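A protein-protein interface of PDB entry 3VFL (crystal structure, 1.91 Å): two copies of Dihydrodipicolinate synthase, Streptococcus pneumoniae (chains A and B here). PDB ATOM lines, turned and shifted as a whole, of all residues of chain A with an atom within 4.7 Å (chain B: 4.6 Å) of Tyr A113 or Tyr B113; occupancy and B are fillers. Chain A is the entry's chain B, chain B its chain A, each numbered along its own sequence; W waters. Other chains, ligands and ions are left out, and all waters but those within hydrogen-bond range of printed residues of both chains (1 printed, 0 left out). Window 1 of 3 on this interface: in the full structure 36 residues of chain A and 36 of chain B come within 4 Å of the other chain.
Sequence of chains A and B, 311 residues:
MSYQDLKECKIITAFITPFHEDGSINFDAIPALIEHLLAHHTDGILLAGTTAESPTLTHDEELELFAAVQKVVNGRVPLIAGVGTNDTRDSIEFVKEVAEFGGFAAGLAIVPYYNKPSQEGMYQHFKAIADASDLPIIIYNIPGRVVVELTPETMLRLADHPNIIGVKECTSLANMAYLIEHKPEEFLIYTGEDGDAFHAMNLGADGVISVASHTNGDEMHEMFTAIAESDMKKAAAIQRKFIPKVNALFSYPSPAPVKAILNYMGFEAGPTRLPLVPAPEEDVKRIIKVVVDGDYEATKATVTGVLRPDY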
ATOM      1  N   THR A  85      31.743  -3.533  26.225  1.00  0.00           N
ATOM      2  CA  THR A  85      31.425  -2.339  25.503  1.00  0.00           C
ATOM      3  C   THR A  85      29.935  -2.348  25.168  1.00  0.00           C
ATOM      4  O   THR A  85      29.145  -3.147  25.742  1.00  0.00           O
ATOM      5  CB  THR A  85      32.212  -2.224  24.144  1.00  0.00           C
ATOM      6  OG1 THR A  85      31.676  -3.183  23.209  1.00  0.00           O
ATOM      7  CG2 THR A  85      33.704  -2.454  24.328  1.00  0.00           C
ATOM      8  N   ASN A  86      29.507  -1.469  24.276  1.00  0.00           N
ATOM      9  CA  ASN A  86      28.117  -1.390  23.961  1.00  0.00           C
ATOM     10  C   ASN A  86      27.735  -2.307  22.788  1.00  0.00           C
ATOM     11  O   ASN A  86      26.618  -2.207  22.237  1.00  0.00           O
ATOM     12  CB  ASN A  86      27.622   0.072  23.728  1.00  0.00           C
ATOM     13  CG  ASN A  86      28.179   0.717  22.477  1.00  0.00           C
ATOM     14  OD1 ASN A  86      29.196   0.301  21.895  1.00  0.00           O
ATOM     15  ND2 ASN A  86      27.521   1.747  22.061  1.00  0.00           N
ATOM     16  N   ILE A 110      30.278  -2.781  31.406  1.00  0.00           N
ATOM     17  CA  ILE A 110      29.427  -1.608  31.662  1.00  0.00           C
ATOM     18  C   ILE A 110      28.047  -1.761  31.043  1.00  0.00           C
ATOM     19  O   ILE A 110      27.881  -2.462  30.035  1.00  0.00           O
ATOM     20  CB  ILE A 110      30.099  -0.321  31.127  1.00  0.00           C
ATOM     21  CG1 ILE A 110      29.464   0.889  31.825  1.00  0.00           C
ATOM     22  CG2 ILE A 110      29.977  -0.255  29.573  1.00  0.00           C
ATOM     23  CD1 ILE A 110      29.983   2.234  31.400  1.00  0.00           C
ATOM     24  N   VAL A 111      27.043  -1.116  31.610  1.00  0.00           N
ATOM     25  CA  VAL A 111      25.724  -1.102  30.934  1.00  0.00           C
ATOM     26  C   VAL A 111      25.951  -0.303  29.621  1.00  0.00           C
ATOM     27  O   VAL A 111      26.581   0.778  29.625  1.00  0.00           O
ATOM     28  CB  VAL A 111      24.626  -0.437  31.781  1.00  0.00           C
ATOM     29  CG1 VAL A 111      23.374  -0.056  30.908  1.00  0.00           C
ATOM     30  CG2 VAL A 111      24.168  -1.267  32.980  1.00  0.00           C
ATOM     31  N   PRO A 112      25.432  -0.832  28.508  1.00  0.00           N
ATOM     32  CA  PRO A 112      25.714  -0.231  27.213  1.00  0.00           C
ATOM     33  C   PRO A 112      25.364   1.262  27.165  1.00  0.00           C
ATOM     34  O   PRO A 112      24.228   1.706  27.534  1.00  0.00           O
ATOM     35  CB  PRO A 112      24.875  -1.060  26.291  1.00  0.00           C
ATOM     36  CG  PRO A 112      25.077  -2.461  26.900  1.00  0.00           C
ATOM     37  CD  PRO A 112      24.965  -2.237  28.380  1.00  0.00           C
ATOM     38  N   TYR A 113      26.341   2.012  26.679  1.00  0.00           N
ATOM     39  CA  TYR A 113      26.227   3.475  26.423  1.00  0.00           C
ATOM     40  C   TYR A 113      25.785   3.744  24.966  1.00  0.00           C
ATOM     41  O   TYR A 113      25.984   2.879  24.069  1.00  0.00           O
ATOM     42  CB  TYR A 113      27.613   4.132  26.747  1.00  0.00           C
ATOM     43  CG  TYR A 113      28.732   3.346  26.197  1.00  0.00           C
ATOM     44  CD1 TYR A 113      29.477   2.511  27.018  1.00  0.00           C
ATOM     45  CD2 TYR A 113      29.090   3.446  24.812  1.00  0.00           C
ATOM     46  CE1 TYR A 113      30.504   1.760  26.532  1.00  0.00           C
ATOM     47  CE2 TYR A 113      30.127   2.680  24.315  1.00  0.00           C
ATOM     48  CZ  TYR A 113      30.849   1.855  25.203  1.00  0.00           C
ATOM     49  OH  TYR A 113      31.872   1.035  24.740  1.00  0.00           O
ATOM     50  N   TYR A 114      25.241   4.953  24.739  1.00  0.00           N
ATOM     51  CA  TYR A 114      24.837   5.406  23.395  1.00  0.00           C
ATOM     52  C   TYR A 114      23.526   4.778  22.834  1.00  0.00           C
ATOM     53  O   TYR A 114      22.568   5.509  22.545  1.00  0.00           O
ATOM     54  CB  TYR A 114      26.028   5.260  22.445  1.00  0.00           C
ATOM     55  CG  TYR A 114      25.842   5.770  21.040  1.00  0.00           C
ATOM     56  CD1 TYR A 114      24.914   6.794  20.744  1.00  0.00           C
ATOM     57  CD2 TYR A 114      26.669   5.292  20.002  1.00  0.00           C
ATOM     58  CE1 TYR A 114      24.755   7.232  19.459  1.00  0.00           C
ATOM     59  CE2 TYR A 114      26.498   5.728  18.685  1.00  0.00           C
ATOM     60  CZ  TYR A 114      25.551   6.700  18.431  1.00  0.00           C
ATOM     61  OH  TYR A 114      25.403   7.209  17.164  1.00  0.00           O
ATOM     62  N   ASN A 115      23.472   3.443  22.733  1.00  0.00           N
ATOM     63  CA  ASN A 115      22.322   2.752  22.085  1.00  0.00           C
ATOM     64  C   ASN A 115      21.127   2.520  23.043  1.00  0.00           C
ATOM     65  O   ASN A 115      20.037   2.179  22.634  1.00  0.00           O
ATOM     66  CB  ASN A 115      22.795   1.468  21.332  1.00  0.00           C
ATOM     67  CG  ASN A 115      23.693   0.549  22.180  1.00  0.00           C
ATOM     68  OD1 ASN A 115      23.811   0.620  23.447  1.00  0.00           O
ATOM     69  ND2 ASN A 115      24.254  -0.405  21.481  1.00  0.00           N
ATOM     70  N   LYS A 116      21.306   2.810  24.317  1.00  0.00           N
ATOM     71  CA  LYS A 116      20.102   2.893  25.260  1.00  0.00           C
ATOM     72  C   LYS A 116      19.179   1.705  25.207  1.00  0.00           C
ATOM     73  O   LYS A 116      17.968   1.812  24.886  1.00  0.00           O
ATOM     74  CB  LYS A 116      19.309   4.192  25.064  1.00  0.00           C
ATOM     75  CG  LYS A 116      20.117   5.475  25.321  1.00  0.00           C
ATOM     76  CD  LYS A 116      19.294   6.747  25.035  1.00  0.00           C
ATOM     77  CE  LYS A 116      18.314   7.184  26.079  1.00  0.00           C
ATOM     78  NZ  LYS A 116      17.621   8.488  25.645  1.00  0.00           N
ATOM     79  N   VAL A 146      26.033   6.618  31.040  1.00  0.00           N
ATOM     80  CA  VAL A 146      25.476   5.854  29.922  1.00  0.00           C
ATOM     81  C   VAL A 146      23.969   6.097  29.661  1.00  0.00           C
ATOM     82  O   VAL A 146      23.383   5.411  28.814  1.00  0.00           O
ATOM     83  CB  VAL A 146      25.776   4.329  30.120  1.00  0.00           C
ATOM     84  CG1 VAL A 146      27.252   4.101  30.387  1.00  0.00           C
ATOM     85  CG2 VAL A 146      24.977   3.704  31.277  1.00  0.00           C
ATOM     86  N   THR B  85      33.258   8.295  16.557  1.00  0.00           N
ATOM     87  CA  THR B  85      33.084   7.476  17.732  1.00  0.00           C
ATOM     88  C   THR B  85      33.555   8.393  18.863  1.00  0.00           C
ATOM     89  O   THR B  85      33.692   9.608  18.655  1.00  0.00           O
ATOM     90  CB  THR B  85      33.962   6.215  17.733  1.00  0.00           C
ATOM     91  OG1 THR B  85      35.375   6.587  17.812  1.00  0.00           O
ATOM     92  CG2 THR B  85      33.648   5.338  16.485  1.00  0.00           C
ATOM     93  N   ASN B  86      33.751   7.815  20.046  1.00  0.00           N
ATOM     94  CA  ASN B  86      34.114   8.626  21.221  1.00  0.00           C
ATOM     95  C   ASN B  86      35.628   8.615  21.314  1.00  0.00           C
ATOM     96  O   ASN B  86      36.167   8.990  22.328  1.00  0.00           O
ATOM     97  CB  ASN B  86      33.442   8.095  22.546  1.00  0.00           C
ATOM     98  CG  ASN B  86      33.750   6.637  22.816  1.00  0.00           C
ATOM     99  OD1 ASN B  86      34.282   5.936  21.915  1.00  0.00           O
ATOM    100  ND2 ASN B  86      33.464   6.158  24.052  1.00  0.00           N
ATOM    101  N   ILE B 110      29.281  12.277  16.124  1.00  0.00           N
ATOM    102  CA  ILE B 110      28.503  12.511  17.381  1.00  0.00           C
ATOM    103  C   ILE B 110      29.410  13.092  18.444  1.00  0.00           C
ATOM    104  O   ILE B 110      30.620  12.829  18.496  1.00  0.00           O
ATOM    105  CB  ILE B 110      27.892  11.190  17.879  1.00  0.00           C
ATOM    106  CG1 ILE B 110      26.852  11.467  19.016  1.00  0.00           C
ATOM    107  CG2 ILE B 110      28.962  10.203  18.325  1.00  0.00           C
ATOM    108  CD1 ILE B 110      25.815  10.415  19.213  1.00  0.00           C
ATOM    109  N   VAL B 111      28.841  13.945  19.269  1.00  0.00           N
ATOM    110  CA  VAL B 111      29.543  14.359  20.516  1.00  0.00           C
ATOM    111  C   VAL B 111      29.968  13.122  21.285  1.00  0.00           C
ATOM    112  O   VAL B 111      29.192  12.238  21.443  1.00  0.00           O
ATOM    113  CB  VAL B 111      28.644  15.256  21.395  1.00  0.00           C
ATOM    114  CG1 VAL B 111      29.263  15.381  22.789  1.00  0.00           C
ATOM    115  CG2 VAL B 111      28.442  16.676  20.869  1.00  0.00           C
ATOM    116  N   PRO B 112      31.258  12.982  21.700  1.00  0.00           N
ATOM    117  CA  PRO B 112      31.665  11.691  22.280  1.00  0.00           C
ATOM    118  C   PRO B 112      30.780  11.191  23.458  1.00  0.00           C
ATOM    119  O   PRO B 112      30.468  11.975  24.379  1.00  0.00           O
ATOM    120  CB  PRO B 112      33.089  12.008  22.767  1.00  0.00           C
ATOM    121  CG  PRO B 112      33.588  12.911  21.653  1.00  0.00           C
ATOM    122  CD  PRO B 112      32.427  13.870  21.517  1.00  0.00           C
ATOM    123  N   TYR B 113      30.324   9.935  23.385  1.00  0.00           N
ATOM    124  CA  TYR B 113      29.499   9.316  24.459  1.00  0.00           C
ATOM    125  C   TYR B 113      30.392   8.656  25.534  1.00  0.00           C
ATOM    126  O   TYR B 113      31.590   8.425  25.309  1.00  0.00           O
ATOM    127  CB  TYR B 113      28.561   8.232  23.814  1.00  0.00           C
ATOM    128  CG  TYR B 113      29.270   7.406  22.761  1.00  0.00           C
ATOM    129  CD1 TYR B 113      29.219   7.808  21.434  1.00  0.00           C
ATOM    130  CD2 TYR B 113      30.007   6.258  23.090  1.00  0.00           C
ATOM    131  CE1 TYR B 113      29.893   7.126  20.434  1.00  0.00           C
ATOM    132  CE2 TYR B 113      30.667   5.511  22.115  1.00  0.00           C
ATOM    133  CZ  TYR B 113      30.600   5.999  20.772  1.00  0.00           C
ATOM    134  OH  TYR B 113      31.204   5.444  19.731  1.00  0.00           O
ATOM    135  N   TYR B 114      29.837   8.338  26.706  1.00  0.00           N
ATOM    136  CA  TYR B 114      30.605   7.581  27.731  1.00  0.00           C
ATOM    137  C   TYR B 114      31.744   8.341  28.486  1.00  0.00           C
ATOM    138  O   TYR B 114      31.661   8.496  29.711  1.00  0.00           O
ATOM    139  CB  TYR B 114      31.076   6.202  27.185  1.00  0.00           C
ATOM    140  CG  TYR B 114      31.802   5.323  28.199  1.00  0.00           C
ATOM    141  CD1 TYR B 114      31.497   5.390  29.566  1.00  0.00           C
ATOM    142  CD2 TYR B 114      32.793   4.412  27.766  1.00  0.00           C
ATOM    143  CE1 TYR B 114      32.181   4.607  30.501  1.00  0.00           C
ATOM    144  CE2 TYR B 114      33.469   3.588  28.655  1.00  0.00           C
ATOM    145  CZ  TYR B 114      33.175   3.678  30.016  1.00  0.00           C
ATOM    146  OH  TYR B 114      33.853   2.848  30.862  1.00  0.00           O
ATOM    147  N   ASN B 115      32.704   8.924  27.763  1.00  0.00           N
ATOM    148  CA  ASN B 115      33.922   9.559  28.411  1.00  0.00           C
ATOM    149  C   ASN B 115      33.661  11.020  28.808  1.00  0.00           C
ATOM    150  O   ASN B 115      34.421  11.609  29.573  1.00  0.00           O
ATOM    151  CB  ASN B 115      35.241   9.371  27.604  1.00  0.00           C
ATOM    152  CG  ASN B 115      35.056   9.581  26.138  1.00  0.00           C
ATOM    153  OD1 ASN B 115      34.058  10.210  25.695  1.00  0.00           O
ATOM    154  ND2 ASN B 115      35.950   9.019  25.334  1.00  0.00           N
ATOM    155  N   LYS B 116      32.519  11.574  28.350  1.00  0.00           N
ATOM    156  CA  LYS B 116      31.997  12.848  28.854  1.00  0.00           C
ATOM    157  C   LYS B 116      33.000  14.006  28.764  1.00  0.00           C
ATOM    158  O   LYS B 116      33.305  14.663  29.771  1.00  0.00           O
ATOM    159  CB  LYS B 116      31.433  12.682  30.319  1.00  0.00           C
ATOM    160  CG  LYS B 116      30.228  11.710  30.230  1.00  0.00           C
ATOM    161  CD  LYS B 116      29.591  11.413  31.555  1.00  0.00           C
ATOM    162  CE  LYS B 116      29.513  12.667  32.393  1.00  0.00           C
ATOM    163  NZ  LYS B 116      28.941  12.263  33.721  1.00  0.00           N
ATOM    164  N   VAL B 146      24.129  11.031  24.840  1.00  0.00           N
ATOM    165  CA  VAL B 146      25.571  11.109  25.190  1.00  0.00           C
ATOM    166  C   VAL B 146      25.920  11.758  26.557  1.00  0.00           C
ATOM    167  O   VAL B 146      27.173  11.825  26.899  1.00  0.00           O
ATOM    168  CB  VAL B 146      26.459  11.658  24.010  1.00  0.00           C
ATOM    169  CG1 VAL B 146      26.160  10.902  22.717  1.00  0.00           C
ATOM    170  CG2 VAL B 146      26.265  13.127  23.691  1.00  0.00           C
HETATM  171  O   HOH W   1      33.902   3.391  24.722  1.00  0.00           O
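OD1 of Asn B115 sits close to O of Tyr B113, 3.1 Å away. ND2 of Asn A86 lies within hydrogen-bond range of O of Tyr A113. The backbone carbonyl oxygen (O) of Tyr B113 sits at hydrogen-bond distance from the side-chain amide nitrogen (ND2) of Asn B86 (3.2 Å). The backbone carbonyl oxygen (O) of Tyr A113 lies close to the side-chain amide oxygen (OD1) of Asn A115, at 3.2 Å.
Tyr B114 touches Ile A110 (CE1 to CD1, 3.4 Å). CD2 of Tyr B113 touches CD2 of Tyr A113, at 3.4 Å. CE1 of Tyr A113 touches CD2 of Tyr B114, at 3.7 Å. Tyr A114 touches Ile B110 (CE1 to CD1, 3.4 Å). Tyr A114 touches Tyr B113.
Of the printed residues of chain B, Ile A110 touches Tyr B114. Val A111 touches none of the printed residues of chain B. Printed residues of chain B within 4 Å of Tyr A114: Ile B110 and Tyr B113. Printed residues of chain A within 4 Å of Ile B110: Tyr A114. Tyr B113 touches two residues of chain A. Of the printed residues of chain A, Tyr B114 touches Ile A110 and Tyr A113. The nearest printed residue of chain B that does not touch Tyr A113 is Asn B86 (4.8 Å). The nearest printed residue of chain A that does not touch Tyr B113 is Asn A86 (4.9 Å). The nearest printed residue of chain B that does not touch Ile A110 is Asn B115 (8.1 Å).
Of the 10 printed residues of chain A, 3 touch a printed residue of chain B. Hydrophobic or aromatic side chains of chain A that line the printed part of chain B: Ile A110, Tyr A113 and Tyr A114. Among the printed residues, 5 pairs touch across the chains.
Ile A110 touches Tyr B114, and with the chains exchanged Tyr A114 touches Ile B110. Tyr A113 touches its own counterpart, Tyr B113. Tyr A113 touches Tyr B114, and with the chains exchanged Tyr A114 touches Tyr B113. 10 positions are printed for both chains.
Water W1 lies within hydrogen-bond range of the side-chain amide nitrogen (ND2) of Asn B86 (2.9 Å) and the side-chain hydroxyl (OH) of Tyr A113 (3.1 Å).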
